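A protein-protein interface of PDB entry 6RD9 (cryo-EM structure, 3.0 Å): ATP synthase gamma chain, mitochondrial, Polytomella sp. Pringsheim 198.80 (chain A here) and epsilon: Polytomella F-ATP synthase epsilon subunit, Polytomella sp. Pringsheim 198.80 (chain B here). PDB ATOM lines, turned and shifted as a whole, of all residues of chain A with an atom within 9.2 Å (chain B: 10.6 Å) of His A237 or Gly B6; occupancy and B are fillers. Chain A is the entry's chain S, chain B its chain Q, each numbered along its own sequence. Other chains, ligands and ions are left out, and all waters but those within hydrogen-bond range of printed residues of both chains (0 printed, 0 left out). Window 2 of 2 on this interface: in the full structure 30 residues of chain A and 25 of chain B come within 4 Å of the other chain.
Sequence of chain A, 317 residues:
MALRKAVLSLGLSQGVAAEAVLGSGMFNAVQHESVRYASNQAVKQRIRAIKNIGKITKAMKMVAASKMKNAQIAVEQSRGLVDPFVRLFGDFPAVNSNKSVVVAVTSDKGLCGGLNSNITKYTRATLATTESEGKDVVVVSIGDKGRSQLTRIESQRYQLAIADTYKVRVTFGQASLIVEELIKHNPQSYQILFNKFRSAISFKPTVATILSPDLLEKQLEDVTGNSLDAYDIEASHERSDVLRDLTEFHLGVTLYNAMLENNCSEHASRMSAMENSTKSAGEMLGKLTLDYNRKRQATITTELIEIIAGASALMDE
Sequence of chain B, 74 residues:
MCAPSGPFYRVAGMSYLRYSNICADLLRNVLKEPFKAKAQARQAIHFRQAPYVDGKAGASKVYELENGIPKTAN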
ATOM      1  N   ILE A 233      13.944   4.600  12.720  1.00  0.00           N
ATOM      2  CA  ILE A 233      13.819   5.958  13.239  1.00  0.00           C
ATOM      3  C   ILE A 233      13.804   5.913  14.757  1.00  0.00           C
ATOM      4  O   ILE A 233      12.994   5.210  15.366  1.00  0.00           O
ATOM      5  CB  ILE A 233      12.557   6.639  12.705  1.00  0.00           C
ATOM      6  CG1 ILE A 233      12.470   6.497  11.195  1.00  0.00           C
ATOM      7  CG2 ILE A 233      12.553   8.093  13.085  1.00  0.00           C
ATOM      8  CD1 ILE A 233      13.610   7.121  10.463  1.00  0.00           C
ATOM      9  N   GLU A 234      14.696   6.674  15.378  1.00  0.00           N
ATOM     10  CA  GLU A 234      14.768   6.768  16.826  1.00  0.00           C
ATOM     11  C   GLU A 234      14.304   8.136  17.311  1.00  0.00           C
ATOM     12  O   GLU A 234      14.910   8.722  18.197  1.00  0.00           O
ATOM     13  CB  GLU A 234      16.196   6.450  17.275  1.00  0.00           C
ATOM     14  CG  GLU A 234      16.401   5.937  18.700  1.00  0.00           C
ATOM     15  CD  GLU A 234      16.899   7.003  19.648  1.00  0.00           C
ATOM     16  OE1 GLU A 234      17.587   7.931  19.196  1.00  0.00           O
ATOM     17  OE2 GLU A 234      16.601   6.924  20.848  1.00  0.00           O
ATOM     18  N   ALA A 235      13.258   8.681  16.717  1.00  0.00           N
ATOM     19  CA  ALA A 235      12.848  10.010  17.126  1.00  0.00           C
ATOM     20  C   ALA A 235      11.802   9.943  18.223  1.00  0.00           C
ATOM     21  O   ALA A 235      11.347   8.874  18.627  1.00  0.00           O
ATOM     22  CB  ALA A 235      12.299  10.794  15.946  1.00  0.00           C
ATOM     23  N   SER A 236      11.418  11.118  18.707  1.00  0.00           N
ATOM     24  CA  SER A 236      10.300  11.201  19.637  1.00  0.00           C
ATOM     25  C   SER A 236       8.981  10.924  18.929  1.00  0.00           C
ATOM     26  O   SER A 236       8.199  10.073  19.358  1.00  0.00           O
ATOM     27  CB  SER A 236      10.273  12.575  20.295  1.00  0.00           C
ATOM     28  OG  SER A 236       9.133  12.713  21.115  1.00  0.00           O
ATOM     29  N   HIS A 237       8.714  11.644  17.854  1.00  0.00           N
ATOM     30  CA  HIS A 237       7.502  11.550  17.078  1.00  0.00           C
ATOM     31  C   HIS A 237       7.770  10.839  15.754  1.00  0.00           C
ATOM     32  O   HIS A 237       8.732  10.076  15.634  1.00  0.00           O
ATOM     33  CB  HIS A 237       6.921  12.941  16.939  1.00  0.00           C
ATOM     34  CG  HIS A 237       6.416  13.485  18.232  1.00  0.00           C
ATOM     35  ND1 HIS A 237       7.254  13.917  19.235  1.00  0.00           N
ATOM     36  CD2 HIS A 237       5.158  13.639  18.703  1.00  0.00           C
ATOM     37  CE1 HIS A 237       6.535  14.329  20.261  1.00  0.00           C
ATOM     38  NE2 HIS A 237       5.260  14.175  19.962  1.00  0.00           N
ATOM     39  N   GLU A 238       6.875  11.031  14.791  1.00  0.00           N
ATOM     40  CA  GLU A 238       6.828  10.217  13.587  1.00  0.00           C
ATOM     41  C   GLU A 238       8.024  10.472  12.677  1.00  0.00           C
ATOM     42  O   GLU A 238       8.782  11.428  12.843  1.00  0.00           O
ATOM     43  CB  GLU A 238       5.551  10.493  12.803  1.00  0.00           C
ATOM     44  CG  GLU A 238       4.288  10.543  13.634  1.00  0.00           C
ATOM     45  CD  GLU A 238       4.194   9.401  14.615  1.00  0.00           C
ATOM     46  OE1 GLU A 238       4.091   9.679  15.827  1.00  0.00           O
ATOM     47  OE2 GLU A 238       4.248   8.235  14.174  1.00  0.00           O
ATOM     48  N   ARG A 239       8.171   9.586  11.690  1.00  0.00           N
ATOM     49  CA  ARG A 239       9.199   9.756  10.673  1.00  0.00           C
ATOM     50  C   ARG A 239       8.922  10.978   9.816  1.00  0.00           C
ATOM     51  O   ARG A 239       9.846  11.705   9.439  1.00  0.00           O
ATOM     52  CB  ARG A 239       9.277   8.517   9.795  1.00  0.00           C
ATOM     53  CG  ARG A 239      10.398   8.565   8.802  1.00  0.00           C
ATOM     54  CD  ARG A 239      10.441   7.329   7.977  1.00  0.00           C
ATOM     55  NE  ARG A 239       9.334   7.297   7.039  1.00  0.00           N
ATOM     56  CZ  ARG A 239       9.282   6.485   5.996  1.00  0.00           C
ATOM     57  NH1 ARG A 239      10.277   5.641   5.772  1.00  0.00           N
ATOM     58  NH2 ARG A 239       8.239   6.515   5.184  1.00  0.00           N
ATOM     59  N   SER A 240       7.650  11.243   9.525  1.00  0.00           N
ATOM     60  CA  SER A 240       7.274  12.453   8.808  1.00  0.00           C
ATOM     61  C   SER A 240       7.513  13.707   9.629  1.00  0.00           C
ATOM     62  O   SER A 240       7.504  14.808   9.077  1.00  0.00           O
ATOM     63  CB  SER A 240       5.804  12.386   8.406  1.00  0.00           C
ATOM     64  OG  SER A 240       4.975  12.442   9.552  1.00  0.00           O
ATOM     65  N   ASP A 241       7.703  13.561  10.931  1.00  0.00           N
ATOM     66  CA  ASP A 241       7.941  14.663  11.840  1.00  0.00           C
ATOM     67  C   ASP A 241       9.425  14.875  12.087  1.00  0.00           C
ATOM     68  O   ASP A 241       9.865  16.010  12.289  1.00  0.00           O
ATOM     69  CB  ASP A 241       7.222  14.369  13.146  1.00  0.00           C
ATOM     70  CG  ASP A 241       6.796  15.599  13.851  1.00  0.00           C
ATOM     71  OD1 ASP A 241       7.599  16.538  14.008  1.00  0.00           O
ATOM     72  OD2 ASP A 241       5.608  15.632  14.209  1.00  0.00           O
ATOM     73  N   VAL A 242      10.211  13.798  12.073  1.00  0.00           N
ATOM     74  CA  VAL A 242      11.649  13.965  12.217  1.00  0.00           C
ATOM     75  C   VAL A 242      12.236  14.484  10.916  1.00  0.00           C
ATOM     76  O   VAL A 242      13.187  15.264  10.942  1.00  0.00           O
ATOM     77  CB  VAL A 242      12.322  12.659  12.701  1.00  0.00           C
ATOM     78  CG1 VAL A 242      12.347  11.584  11.654  1.00  0.00           C
ATOM     79  CG2 VAL A 242      13.706  12.907  13.149  1.00  0.00           C
ATOM     80  N   LEU A 243      11.635  14.146   9.770  1.00  0.00           N
ATOM     81  CA  LEU A 243      12.108  14.675   8.495  1.00  0.00           C
ATOM     82  C   LEU A 243      11.773  16.144   8.344  1.00  0.00           C
ATOM     83  O   LEU A 243      12.444  16.853   7.593  1.00  0.00           O
ATOM     84  CB  LEU A 243      11.513  13.887   7.336  1.00  0.00           C
ATOM     85  CG  LEU A 243      12.417  12.885   6.641  1.00  0.00           C
ATOM     86  CD1 LEU A 243      12.765  11.755   7.553  1.00  0.00           C
ATOM     87  CD2 LEU A 243      11.706  12.354   5.430  1.00  0.00           C
ATOM     88  N   ARG A 244      10.736  16.609   9.029  1.00  0.00           N
ATOM     89  CA  ARG A 244      10.509  18.039   9.138  1.00  0.00           C
ATOM     90  C   ARG A 244      11.631  18.700   9.925  1.00  0.00           C
ATOM     91  O   ARG A 244      12.079  19.789   9.572  1.00  0.00           O
ATOM     92  CB  ARG A 244       9.148  18.291   9.779  1.00  0.00           C
ATOM     93  CG  ARG A 244       8.858  19.717  10.159  1.00  0.00           C
ATOM     94  CD  ARG A 244       8.747  20.592   8.949  1.00  0.00           C
ATOM     95  NE  ARG A 244       7.550  20.299   8.175  1.00  0.00           N
ATOM     96  CZ  ARG A 244       7.206  20.947   7.069  1.00  0.00           C
ATOM     97  NH1 ARG A 244       6.098  20.613   6.422  1.00  0.00           N
ATOM     98  NH2 ARG A 244       7.977  21.922   6.606  1.00  0.00           N
ATOM     99  N   ASP A 245      12.124  18.041  10.972  1.00  0.00           N
ATOM    100  CA  ASP A 245      13.250  18.590  11.718  1.00  0.00           C
ATOM    101  C   ASP A 245      14.543  18.468  10.929  1.00  0.00           C
ATOM    102  O   ASP A 245      15.442  19.301  11.065  1.00  0.00           O
ATOM    103  CB  ASP A 245      13.402  17.874  13.059  1.00  0.00           C
ATOM    104  CG  ASP A 245      12.252  18.139  14.008  1.00  0.00           C
ATOM    105  OD1 ASP A 245      11.613  19.203  13.909  1.00  0.00           O
ATOM    106  OD2 ASP A 245      11.999  17.279  14.875  1.00  0.00           O
ATOM    107  N   ALA B   3      -1.589  23.572  17.900  1.00  0.00           N
ATOM    108  CA  ALA B   3      -2.089  23.459  16.532  1.00  0.00           C
ATOM    109  C   ALA B   3      -1.159  22.709  15.547  1.00  0.00           C
ATOM    110  O   ALA B   3      -1.673  22.048  14.644  1.00  0.00           O
ATOM    111  CB  ALA B   3      -2.444  24.852  15.986  1.00  0.00           C
ATOM    112  N   PRO B   4       0.171  22.789  15.672  1.00  0.00           N
ATOM    113  CA  PRO B   4       0.998  21.753  15.052  1.00  0.00           C
ATOM    114  C   PRO B   4       1.125  20.558  15.980  1.00  0.00           C
ATOM    115  O   PRO B   4       0.894  20.646  17.185  1.00  0.00           O
ATOM    116  CB  PRO B   4       2.357  22.435  14.841  1.00  0.00           C
ATOM    117  CG  PRO B   4       2.094  23.883  15.004  1.00  0.00           C
ATOM    118  CD  PRO B   4       1.030  23.933  16.043  1.00  0.00           C
ATOM    119  N   SER B   5       1.496  19.429  15.391  1.00  0.00           N
ATOM    120  CA  SER B   5       1.617  18.169  16.109  1.00  0.00           C
ATOM    121  C   SER B   5       3.042  17.664  15.969  1.00  0.00           C
ATOM    122  O   SER B   5       3.543  17.520  14.851  1.00  0.00           O
ATOM    123  CB  SER B   5       0.621  17.142  15.575  1.00  0.00           C
ATOM    124  OG  SER B   5       0.909  16.798  14.233  1.00  0.00           O
ATOM    125  N   GLY B   6       3.688  17.399  17.095  1.00  0.00           N
ATOM    126  CA  GLY B   6       5.045  16.917  17.092  1.00  0.00           C
ATOM    127  C   GLY B   6       5.741  17.127  18.414  1.00  0.00           C
ATOM    128  O   GLY B   6       5.128  17.061  19.482  1.00  0.00           O
ATOM    129  N   PRO B   7       7.042  17.397  18.368  1.00  0.00           N
ATOM    130  CA  PRO B   7       7.794  17.607  19.609  1.00  0.00           C
ATOM    131  C   PRO B   7       7.464  18.917  20.301  1.00  0.00           C
ATOM    132  O   PRO B   7       6.641  19.695  19.815  1.00  0.00           O
ATOM    133  CB  PRO B   7       9.252  17.568  19.142  1.00  0.00           C
ATOM    134  CG  PRO B   7       9.212  16.933  17.793  1.00  0.00           C
ATOM    135  CD  PRO B   7       7.925  17.313  17.198  1.00  0.00           C
ATOM    136  N   PHE B   8       8.103  19.166  21.445  1.00  0.00           N
ATOM    137  CA  PHE B   8       7.697  20.282  22.286  1.00  0.00           C
ATOM    138  C   PHE B   8       8.080  21.624  21.696  1.00  0.00           C
ATOM    139  O   PHE B   8       7.478  22.640  22.056  1.00  0.00           O
ATOM    140  CB  PHE B   8       8.283  20.144  23.689  1.00  0.00           C
ATOM    141  CG  PHE B   8       9.780  20.181  23.747  1.00  0.00           C
ATOM    142  CD1 PHE B   8      10.444  21.354  24.055  1.00  0.00           C
ATOM    143  CD2 PHE B   8      10.523  19.029  23.554  1.00  0.00           C
ATOM    144  CE1 PHE B   8      11.814  21.383  24.130  1.00  0.00           C
ATOM    145  CE2 PHE B   8      11.890  19.053  23.628  1.00  0.00           C
ATOM    146  CZ  PHE B   8      12.537  20.229  23.920  1.00  0.00           C
ATOM    147  N   TYR B   9       9.063  21.656  20.811  1.00  0.00           N
ATOM    148  CA  TYR B   9       9.371  22.879  20.093  1.00  0.00           C
ATOM    149  C   TYR B   9       8.442  23.070  18.909  1.00  0.00           C
ATOM    150  O   TYR B   9       8.051  24.197  18.606  1.00  0.00           O
ATOM    151  CB  TYR B   9      10.832  22.871  19.632  1.00  0.00           C
ATOM    152  CG  TYR B   9      11.290  21.597  18.970  1.00  0.00           C
ATOM    153  CD1 TYR B   9      11.893  20.592  19.704  1.00  0.00           C
ATOM    154  CD2 TYR B   9      11.145  21.412  17.605  1.00  0.00           C
ATOM    155  CE1 TYR B   9      12.317  19.439  19.102  1.00  0.00           C
ATOM    156  CE2 TYR B   9      11.562  20.260  17.001  1.00  0.00           C
ATOM    157  CZ  TYR B   9      12.146  19.281  17.751  1.00  0.00           C
ATOM    158  OH  TYR B   9      12.567  18.131  17.144  1.00  0.00           O
ATOM    159  N   ARG B  10       8.051  21.979  18.256  1.00  0.00           N
ATOM    160  CA  ARG B  10       7.273  22.094  17.032  1.00  0.00           C
ATOM    161  C   ARG B  10       5.821  22.447  17.315  1.00  0.00           C
ATOM    162  O   ARG B  10       5.214  23.203  16.551  1.00  0.00           O
ATOM    163  CB  ARG B  10       7.367  20.797  16.243  1.00  0.00           C
ATOM    164  CG  ARG B  10       6.834  20.882  14.851  1.00  0.00           C
ATOM    165  CD  ARG B  10       7.679  21.801  14.013  1.00  0.00           C
ATOM    166  NE  ARG B  10       8.996  21.242  13.737  1.00  0.00           N
ATOM    167  CZ  ARG B  10       9.821  21.727  12.818  1.00  0.00           C
ATOM    168  NH1 ARG B  10       9.450  22.764  12.085  1.00  0.00           N
ATOM    169  NH2 ARG B  10      11.002  21.170  12.615  1.00  0.00           N
ATOM    170  N   VAL B  11       5.253  21.937  18.412  1.00  0.00           N
ATOM    171  CA  VAL B  11       3.896  22.328  18.779  1.00  0.00           C
ATOM    172  C   VAL B  11       3.851  23.738  19.347  1.00  0.00           C
ATOM    173  O   VAL B  11       2.783  24.360  19.352  1.00  0.00           O
ATOM    174  CB  VAL B  11       3.256  21.345  19.779  1.00  0.00           C
ATOM    175  CG1 VAL B  11       3.349  19.940  19.262  1.00  0.00           C
ATOM    176  CG2 VAL B  11       3.910  21.435  21.147  1.00  0.00           C
ATOM    177  N   ALA B  12       4.983  24.269  19.800  1.00  0.00           N
ATOM    178  CA  ALA B  12       5.067  25.634  20.284  1.00  0.00           C
ATOM    179  C   ALA B  12       5.397  26.623  19.177  1.00  0.00           C
ATOM    180  O   ALA B  12       5.805  27.750  19.472  1.00  0.00           O
ATOM    181  CB  ALA B  12       6.104  25.735  21.402  1.00  0.00           C
ATOM    182  N   GLY B  13       5.256  26.220  17.914  1.00  0.00           N
ATOM    183  CA  GLY B  13       5.528  27.076  16.779  1.00  0.00           C
ATOM    184  C   GLY B  13       6.988  27.208  16.412  1.00  0.00           C
ATOM    185  O   GLY B  13       7.291  27.700  15.319  1.00  0.00           O
ATOM    186  N   MET B  14       7.896  26.772  17.277  1.00  0.00           N
ATOM    187  CA  MET B  14       9.321  26.944  17.051  1.00  0.00           C
ATOM    188  C   MET B  14       9.824  25.915  16.048  1.00  0.00           C
ATOM    189  O   MET B  14       9.397  24.760  16.056  1.00  0.00           O
ATOM    190  CB  MET B  14      10.060  26.816  18.379  1.00  0.00           C
ATOM    191  CG  MET B  14      11.520  27.130  18.326  1.00  0.00           C
ATOM    192  SD  MET B  14      12.374  26.618  19.817  1.00  0.00           S
ATOM    193  CE  MET B  14      11.312  27.259  21.079  1.00  0.00           C
ATOM    194  N   TYR B  16      12.900  23.584  14.256  1.00  0.00           N
ATOM    195  CA  TYR B  16      13.969  22.780  14.833  1.00  0.00           C
ATOM    196  C   TYR B  16      15.285  23.541  14.841  1.00  0.00           C
ATOM    197  O   TYR B  16      16.104  23.358  15.747  1.00  0.00           O
ATOM    198  CB  TYR B  16      14.121  21.465  14.074  1.00  0.00           C
ATOM    199  CG  TYR B  16      15.296  20.665  14.556  1.00  0.00           C
ATOM    200  CD1 TYR B  16      15.243  19.991  15.756  1.00  0.00           C
ATOM    201  CD2 TYR B  16      16.476  20.612  13.828  1.00  0.00           C
ATOM    202  CE1 TYR B  16      16.317  19.282  16.214  1.00  0.00           C
ATOM    203  CE2 TYR B  16      17.555  19.917  14.289  1.00  0.00           C
ATOM    204  CZ  TYR B  16      17.466  19.247  15.475  1.00  0.00           C
ATOM    205  OH  TYR B  16      18.537  18.535  15.932  1.00  0.00           O
ATOM    206  N   TYR B  19      15.383  25.727  17.868  1.00  0.00           N
ATOM    207  CA  TYR B  19      15.501  24.908  19.067  1.00  0.00           C
ATOM    208  C   TYR B  19      16.904  24.347  19.209  1.00  0.00           C
ATOM    209  O   TYR B  19      17.478  24.344  20.302  1.00  0.00           O
ATOM    210  CB  TYR B  19      14.475  23.779  19.025  1.00  0.00           C
ATOM    211  CG  TYR B  19      14.853  22.591  19.869  1.00  0.00           C
ATOM    212  CD1 TYR B  19      15.281  21.410  19.283  1.00  0.00           C
ATOM    213  CD2 TYR B  19      14.785  22.652  21.248  1.00  0.00           C
ATOM    214  CE1 TYR B  19      15.639  20.338  20.046  1.00  0.00           C
ATOM    215  CE2 TYR B  19      15.140  21.582  22.014  1.00  0.00           C
ATOM    216  CZ  TYR B  19      15.565  20.427  21.410  1.00  0.00           C
ATOM    217  OH  TYR B  19      15.919  19.346  22.181  1.00  0.00           O
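Among the printed residues, merely in contact across the chains: Asp A241 with Gly B6 (3.2 Å), Asp A245 with Tyr B16 (3.2 Å), Asp A241 with Pro B7 (3.3 Å), Arg A244 with Arg B10 (3.5 Å) and His A237 with Pro B7 (3.6 Å).
The side-chain carboxylate (OD2) of Asp A241 lies close to the backbone carbonyl oxygen (O) of Ser B5.
A ring nitrogen (NE2) of His A237 is in hydrogen-bond range of the backbone carbonyl oxygen of Gly B6 (2.9 Å).
OD1 of Asp A245 is in salt-bridge range of NH2 of Arg B10 (2.4 Å).
The side-chain hydroxyl (OH) of Tyr B9 sits at hydrogen-bond distance from the side-chain carboxylate (OD2) of Asp A245 (2.5 Å).
Of the 13 printed residues of chain A, 4 touch a printed residue of chain B.
Hydrophobic or aromatic side chains of chain A within 4 Å of the printed part of chain B: His A237.
Of the 14 printed residues of chain B, 6 touch a printed residue of chain A.
Among the printed residues, 9 pairs touch across the chains.
Among the printed residues, Asp or Glu carboxylates within 4 Å of a Lys or Arg side-chain nitrogen of the other chain: Asp A245 with Arg B10 (2.4 Å).
Of chain B, only Gly B6 (2.9 Å) and Pro B7 (3.6 Å) come within 4 Å of His A237.
Gly B6 touches just these residues of chain A: His A237 and Asp A241.
No residue of chain B comes within 4 Å of Ala A235.
No residue of chain B comes within 4 Å of Glu A238.
Ser B5 touches just one residue of chain A: Asp A241.
Pro B7 touches two residues of chain A.
Of the printed residues of chain B, Asp A245 touches Tyr B9 (2.5 Å), Arg B10 (2.4 Å) and Tyr B16 (3.2 Å).
Of the printed residues of chain A, Tyr B9 touches Asp A245.
Val A242 touches none of the printed residues of chain B.
Phe B8 touches none of the printed residues of chain A.
The nearest residue of chain A that does not touch Gly B6 is Ser A236 (6.1 Å).
The backbone carbonyl oxygen (O) of Tyr B9 sits at hydrogen-bond distance from the backbone NH (N) of Met B14, at 2.9 Å.
ND1 of His A237 is in hydrogen-bond range of OG of Ser A236.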
